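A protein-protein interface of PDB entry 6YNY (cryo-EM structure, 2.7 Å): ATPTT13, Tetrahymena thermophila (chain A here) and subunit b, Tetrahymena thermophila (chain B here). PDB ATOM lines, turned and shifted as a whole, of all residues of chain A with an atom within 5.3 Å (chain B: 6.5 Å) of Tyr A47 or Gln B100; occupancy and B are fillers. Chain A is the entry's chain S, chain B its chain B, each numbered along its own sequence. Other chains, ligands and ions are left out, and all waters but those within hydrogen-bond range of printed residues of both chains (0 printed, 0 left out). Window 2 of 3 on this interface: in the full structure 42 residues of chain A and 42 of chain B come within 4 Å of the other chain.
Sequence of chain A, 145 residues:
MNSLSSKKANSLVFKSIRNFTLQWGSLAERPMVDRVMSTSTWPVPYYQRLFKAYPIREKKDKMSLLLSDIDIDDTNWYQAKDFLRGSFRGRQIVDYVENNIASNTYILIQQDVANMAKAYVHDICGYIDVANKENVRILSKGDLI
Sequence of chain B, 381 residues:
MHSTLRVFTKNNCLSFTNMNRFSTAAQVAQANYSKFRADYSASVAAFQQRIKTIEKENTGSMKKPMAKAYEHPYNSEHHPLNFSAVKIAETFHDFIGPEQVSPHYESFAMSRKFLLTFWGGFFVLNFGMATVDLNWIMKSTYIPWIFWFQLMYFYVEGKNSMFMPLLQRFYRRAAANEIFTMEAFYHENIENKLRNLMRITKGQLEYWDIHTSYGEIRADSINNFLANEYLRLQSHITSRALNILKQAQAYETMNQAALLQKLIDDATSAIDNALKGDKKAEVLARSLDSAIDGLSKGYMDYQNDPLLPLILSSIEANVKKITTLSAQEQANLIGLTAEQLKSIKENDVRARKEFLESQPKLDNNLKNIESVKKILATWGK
Tyr A47 touches four residues of chain B.
Of the printed residues of chain B, Leu A50 touches Glu B99.
Of the printed residues of chain A, Glu B99 touches Tyr A47 (2.8 Å), Arg A49 (2.6 Å) and Leu A50 (2.9 Å).
Of chain A, only Tyr A47 comes within 4 Å of Gln B100.
Of the printed residues of chain A, Ser B102 touches Tyr A46 and Tyr A47.
The nearest printed residue of chain A that does not touch Gln B100 is Arg A49 (6.3 Å).
The nearest printed residue of chain A that does not touch Glu B99 is Gln A48 (4.1 Å).
Among the printed residues, merely in contact across the chains: Pro A45 with His B104, Arg A49 with Val B101, Tyr A47 with Ser B102, Tyr A47 with Val B101 and Tyr A47 with Gln B100.
OG of Ser B102 lies close to OH of Tyr A46, at 3.4 Å.
N of Tyr A46 sits at hydrogen-bond distance from O of His B104 (3.4 Å).
The side-chain hydroxyl of Tyr A47 is in hydrogen-bond range of the side-chain carboxylate of Glu B99 (2.8 Å).
The side-chain carboxylate of Glu B99 is in salt-bridge range of the guanidinium group of Arg A49.
N of Leu A50 sits at hydrogen-bond distance from OE2 of Glu B99 (2.9 Å).
Of the 7 printed residues of chain A, 5 touch a printed residue of chain B.
Hydrophobic or aromatic side chains of chain A within 4 Å of the printed part of chain B: Pro A45, Tyr A46, Tyr A47 and Leu A50.
Of the 9 printed residues of chain B, 5 touch a printed residue of chain A.
Printed residues of chain B that touch a printed residue of chain A: Glu B99, Gln B100, Val B101, Ser B102 and His B104.
Among the printed residues, 10 pairs touch across the chains.
Among the printed residues, Asp or Glu carboxylates within 4 Å of a Lys or Arg side-chain nitrogen of the other chain: Arg A49 with Glu B99.
The guanidinium group of Arg A35 is in hydrogen-bond range of the backbone carbonyl oxygen of Pro A45, 3.2 Å away.
NE of Arg A35 sits close to O of Tyr A47 (3.4 Å).
The side-chain hydroxyl (OG) of Ser B102 lies close to the backbone NH (N) of His B104 (3.4 Å).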
ATOM      1  N   ARG A  35      20.872 -25.210 -13.389  1.00  0.00           N
ATOM      2  CA  ARG A  35      20.156 -25.099 -14.650  1.00  0.00           C
ATOM      3  C   ARG A  35      21.092 -24.680 -15.776  1.00  0.00           C
ATOM      4  O   ARG A  35      21.924 -23.783 -15.617  1.00  0.00           O
ATOM      5  CB  ARG A  35      19.024 -24.088 -14.520  1.00  0.00           C
ATOM      6  CG  ARG A  35      18.019 -24.108 -15.652  1.00  0.00           C
ATOM      7  CD  ARG A  35      17.078 -25.283 -15.546  1.00  0.00           C
ATOM      8  NE  ARG A  35      15.876 -25.083 -16.347  1.00  0.00           N
ATOM      9  CZ  ARG A  35      15.678 -25.583 -17.559  1.00  0.00           C
ATOM     10  NH1 ARG A  35      16.600 -26.326 -18.151  1.00  0.00           N
ATOM     11  NH2 ARG A  35      14.544 -25.324 -18.186  1.00  0.00           N
ATOM     12  N   PRO A  45      13.792 -20.315 -15.457  1.00  0.00           N
ATOM     13  CA  PRO A  45      13.440 -21.137 -14.296  1.00  0.00           C
ATOM     14  C   PRO A  45      14.645 -21.909 -13.783  1.00  0.00           C
ATOM     15  O   PRO A  45      15.404 -22.496 -14.554  1.00  0.00           O
ATOM     16  CB  PRO A  45      12.358 -22.069 -14.841  1.00  0.00           C
ATOM     17  CG  PRO A  45      11.784 -21.352 -15.980  1.00  0.00           C
ATOM     18  CD  PRO A  45      12.897 -20.578 -16.596  1.00  0.00           C
ATOM     19  N   TYR A  46      14.808 -21.910 -12.461  1.00  0.00           N
ATOM     20  CA  TYR A  46      16.011 -22.467 -11.861  1.00  0.00           C
ATOM     21  C   TYR A  46      15.973 -23.985 -11.780  1.00  0.00           C
ATOM     22  O   TYR A  46      17.019 -24.630 -11.900  1.00  0.00           O
ATOM     23  CB  TYR A  46      16.220 -21.882 -10.465  1.00  0.00           C
ATOM     24  CG  TYR A  46      15.368 -22.498  -9.385  1.00  0.00           C
ATOM     25  CD1 TYR A  46      15.847 -23.542  -8.613  1.00  0.00           C
ATOM     26  CD2 TYR A  46      14.093 -22.033  -9.128  1.00  0.00           C
ATOM     27  CE1 TYR A  46      15.079 -24.108  -7.631  1.00  0.00           C
ATOM     28  CE2 TYR A  46      13.319 -22.592  -8.143  1.00  0.00           C
ATOM     29  CZ  TYR A  46      13.820 -23.631  -7.394  1.00  0.00           C
ATOM     30  OH  TYR A  46      13.064 -24.209  -6.402  1.00  0.00           O
ATOM     31  N   TYR A  47      14.797 -24.568 -11.583  1.00  0.00           N
ATOM     32  CA  TYR A  47      14.716 -25.981 -11.249  1.00  0.00           C
ATOM     33  C   TYR A  47      15.291 -26.837 -12.366  1.00  0.00           C
ATOM     34  O   TYR A  47      14.920 -26.694 -13.533  1.00  0.00           O
ATOM     35  CB  TYR A  47      13.272 -26.376 -10.973  1.00  0.00           C
ATOM     36  CG  TYR A  47      13.149 -27.689 -10.250  1.00  0.00           C
ATOM     37  CD1 TYR A  47      13.280 -27.755  -8.877  1.00  0.00           C
ATOM     38  CD2 TYR A  47      12.913 -28.864 -10.940  1.00  0.00           C
ATOM     39  CE1 TYR A  47      13.177 -28.949  -8.213  1.00  0.00           C
ATOM     40  CE2 TYR A  47      12.808 -30.061 -10.283  1.00  0.00           C
ATOM     41  CZ  TYR A  47      12.942 -30.099  -8.917  1.00  0.00           C
ATOM     42  OH  TYR A  47      12.838 -31.293  -8.254  1.00  0.00           O
ATOM     43  N   GLN A  48      16.199 -27.733 -11.997  1.00  0.00           N
ATOM     44  CA  GLN A  48      16.763 -28.706 -12.917  1.00  0.00           C
ATOM     45  C   GLN A  48      16.085 -30.045 -12.678  1.00  0.00           C
ATOM     46  O   GLN A  48      16.138 -30.586 -11.569  1.00  0.00           O
ATOM     47  CB  GLN A  48      18.275 -28.817 -12.735  1.00  0.00           C
ATOM     48  CG  GLN A  48      18.937 -29.888 -13.584  1.00  0.00           C
ATOM     49  CD  GLN A  48      18.635 -29.745 -15.056  1.00  0.00           C
ATOM     50  OE1 GLN A  48      18.565 -28.635 -15.582  1.00  0.00           O
ATOM     51  NE2 GLN A  48      18.441 -30.873 -15.735  1.00  0.00           N
ATOM     52  N   ARG A  49      15.446 -30.569 -13.716  1.00  0.00           N
ATOM     53  CA  ARG A  49      14.676 -31.796 -13.593  1.00  0.00           C
ATOM     54  C   ARG A  49      15.598 -32.971 -13.310  1.00  0.00           C
ATOM     55  O   ARG A  49      16.639 -33.131 -13.952  1.00  0.00           O
ATOM     56  CB  ARG A  49      13.872 -32.033 -14.867  1.00  0.00           C
ATOM     57  CG  ARG A  49      12.661 -31.139 -14.984  1.00  0.00           C
ATOM     58  CD  ARG A  49      11.526 -31.657 -14.143  1.00  0.00           C
ATOM     59  NE  ARG A  49      10.666 -32.561 -14.894  1.00  0.00           N
ATOM     60  CZ  ARG A  49       9.947 -33.534 -14.351  1.00  0.00           C
ATOM     61  NH1 ARG A  49       9.978 -33.750 -13.046  1.00  0.00           N
ATOM     62  NH2 ARG A  49       9.197 -34.302 -15.122  1.00  0.00           N
ATOM     63  N   LEU A  50      15.217 -33.787 -12.331  1.00  0.00           N
ATOM     64  CA  LEU A  50      15.990 -34.964 -11.961  1.00  0.00           C
ATOM     65  C   LEU A  50      15.573 -36.184 -12.768  1.00  0.00           C
ATOM     66  O   LEU A  50      16.418 -36.863 -13.358  1.00  0.00           O
ATOM     67  CB  LEU A  50      15.816 -35.248 -10.470  1.00  0.00           C
ATOM     68  CG  LEU A  50      16.176 -34.100  -9.540  1.00  0.00           C
ATOM     69  CD1 LEU A  50      15.487 -34.276  -8.215  1.00  0.00           C
ATOM     70  CD2 LEU A  50      17.671 -34.027  -9.360  1.00  0.00           C
ATOM     71  N   ILE B  96       5.280 -40.427  -2.118  1.00  0.00           N
ATOM     72  CA  ILE B  96       5.986 -39.153  -2.110  1.00  0.00           C
ATOM     73  C   ILE B  96       5.530 -38.238  -3.228  1.00  0.00           C
ATOM     74  O   ILE B  96       5.866 -37.050  -3.224  1.00  0.00           O
ATOM     75  CB  ILE B  96       7.510 -39.367  -2.199  1.00  0.00           C
ATOM     76  CG1 ILE B  96       7.878 -40.103  -3.487  1.00  0.00           C
ATOM     77  CG2 ILE B  96       7.993 -40.135  -0.995  1.00  0.00           C
ATOM     78  CD1 ILE B  96       9.338 -40.188  -3.736  1.00  0.00           C
ATOM     79  N   GLY B  97       4.772 -38.761  -4.183  1.00  0.00           N
ATOM     80  CA  GLY B  97       4.210 -37.960  -5.235  1.00  0.00           C
ATOM     81  C   GLY B  97       5.223 -37.604  -6.295  1.00  0.00           C
ATOM     82  O   GLY B  97       6.397 -37.977  -6.222  1.00  0.00           O
ATOM     83  N   PRO B  98       4.781 -36.875  -7.311  1.00  0.00           N
ATOM     84  CA  PRO B  98       5.694 -36.473  -8.378  1.00  0.00           C
ATOM     85  C   PRO B  98       6.719 -35.467  -7.891  1.00  0.00           C
ATOM     86  O   PRO B  98       6.556 -34.805  -6.865  1.00  0.00           O
ATOM     87  CB  PRO B  98       4.765 -35.854  -9.424  1.00  0.00           C
ATOM     88  CG  PRO B  98       3.577 -35.424  -8.663  1.00  0.00           C
ATOM     89  CD  PRO B  98       3.410 -36.403  -7.553  1.00  0.00           C
ATOM     90  N   GLU B  99       7.799 -35.371  -8.653  1.00  0.00           N
ATOM     91  CA  GLU B  99       8.839 -34.394  -8.384  1.00  0.00           C
ATOM     92  C   GLU B  99       8.235 -33.004  -8.300  1.00  0.00           C
ATOM     93  O   GLU B  99       7.626 -32.521  -9.258  1.00  0.00           O
ATOM     94  CB  GLU B  99       9.889 -34.466  -9.491  1.00  0.00           C
ATOM     95  CG  GLU B  99      11.103 -33.603  -9.281  1.00  0.00           C
ATOM     96  CD  GLU B  99      12.092 -33.726 -10.420  1.00  0.00           C
ATOM     97  OE1 GLU B  99      11.817 -34.497 -11.362  1.00  0.00           O
ATOM     98  OE2 GLU B  99      13.142 -33.054 -10.376  1.00  0.00           O
ATOM     99  N   GLN B 100       8.389 -32.364  -7.143  1.00  0.00           N
ATOM    100  CA  GLN B 100       7.809 -31.043  -6.914  1.00  0.00           C
ATOM    101  C   GLN B 100       8.634 -30.016  -7.679  1.00  0.00           C
ATOM    102  O   GLN B 100       9.542 -29.372  -7.153  1.00  0.00           O
ATOM    103  CB  GLN B 100       7.752 -30.727  -5.429  1.00  0.00           C
ATOM    104  CG  GLN B 100       6.953 -31.732  -4.644  1.00  0.00           C
ATOM    105  CD  GLN B 100       6.477 -31.203  -3.319  1.00  0.00           C
ATOM    106  OE1 GLN B 100       6.854 -30.113  -2.897  1.00  0.00           O
ATOM    107  NE2 GLN B 100       5.636 -31.973  -2.656  1.00  0.00           N
ATOM    108  N   VAL B 101       8.300 -29.871  -8.954  1.00  0.00           N
ATOM    109  CA  VAL B 101       9.006 -28.954  -9.835  1.00  0.00           C
ATOM    110  C   VAL B 101       8.583 -27.530  -9.514  1.00  0.00           C
ATOM    111  O   VAL B 101       7.389 -27.213  -9.486  1.00  0.00           O
ATOM    112  CB  VAL B 101       8.730 -29.300 -11.305  1.00  0.00           C
ATOM    113  CG1 VAL B 101       9.382 -28.296 -12.218  1.00  0.00           C
ATOM    114  CG2 VAL B 101       9.224 -30.691 -11.614  1.00  0.00           C
ATOM    115  N   SER B 102       9.564 -26.673  -9.264  1.00  0.00           N
ATOM    116  CA  SER B 102       9.304 -25.266  -9.021  1.00  0.00           C
ATOM    117  C   SER B 102       9.226 -24.527 -10.347  1.00  0.00           C
ATOM    118  O   SER B 102      10.175 -24.602 -11.138  1.00  0.00           O
ATOM    119  CB  SER B 102      10.390 -24.661  -8.156  1.00  0.00           C
ATOM    120  OG  SER B 102      10.189 -23.274  -7.979  1.00  0.00           O
ATOM    121  N   PRO B 103       8.132 -23.823 -10.641  1.00  0.00           N
ATOM    122  CA  PRO B 103       8.055 -23.052 -11.884  1.00  0.00           C
ATOM    123  C   PRO B 103       8.685 -21.674 -11.800  1.00  0.00           C
ATOM    124  O   PRO B 103       8.628 -20.927 -12.781  1.00  0.00           O
ATOM    125  CB  PRO B 103       6.547 -22.944 -12.104  1.00  0.00           C
ATOM    126  CG  PRO B 103       5.997 -22.894 -10.744  1.00  0.00           C
ATOM    127  CD  PRO B 103       6.866 -23.763  -9.893  1.00  0.00           C
ATOM    128  N   HIS B 104       9.284 -21.327 -10.672  1.00  0.00           N
ATOM    129  CA  HIS B 104       9.737 -19.973 -10.426  1.00  0.00           C
ATOM    130  C   HIS B 104      11.129 -19.728 -10.988  1.00  0.00           C
ATOM    131  O   HIS B 104      11.853 -20.645 -11.381  1.00  0.00           O
ATOM    132  CB  HIS B 104       9.727 -19.674  -8.931  1.00  0.00           C
ATOM    133  CG  HIS B 104       8.360 -19.600  -8.336  1.00  0.00           C
ATOM    134  ND1 HIS B 104       7.697 -20.706  -7.852  1.00  0.00           N
ATOM    135  CD2 HIS B 104       7.531 -18.550  -8.142  1.00  0.00           C
ATOM    136  CE1 HIS B 104       6.518 -20.339  -7.386  1.00  0.00           C
ATOM    137  NE2 HIS B 104       6.393 -19.036  -7.551  1.00  0.00           N
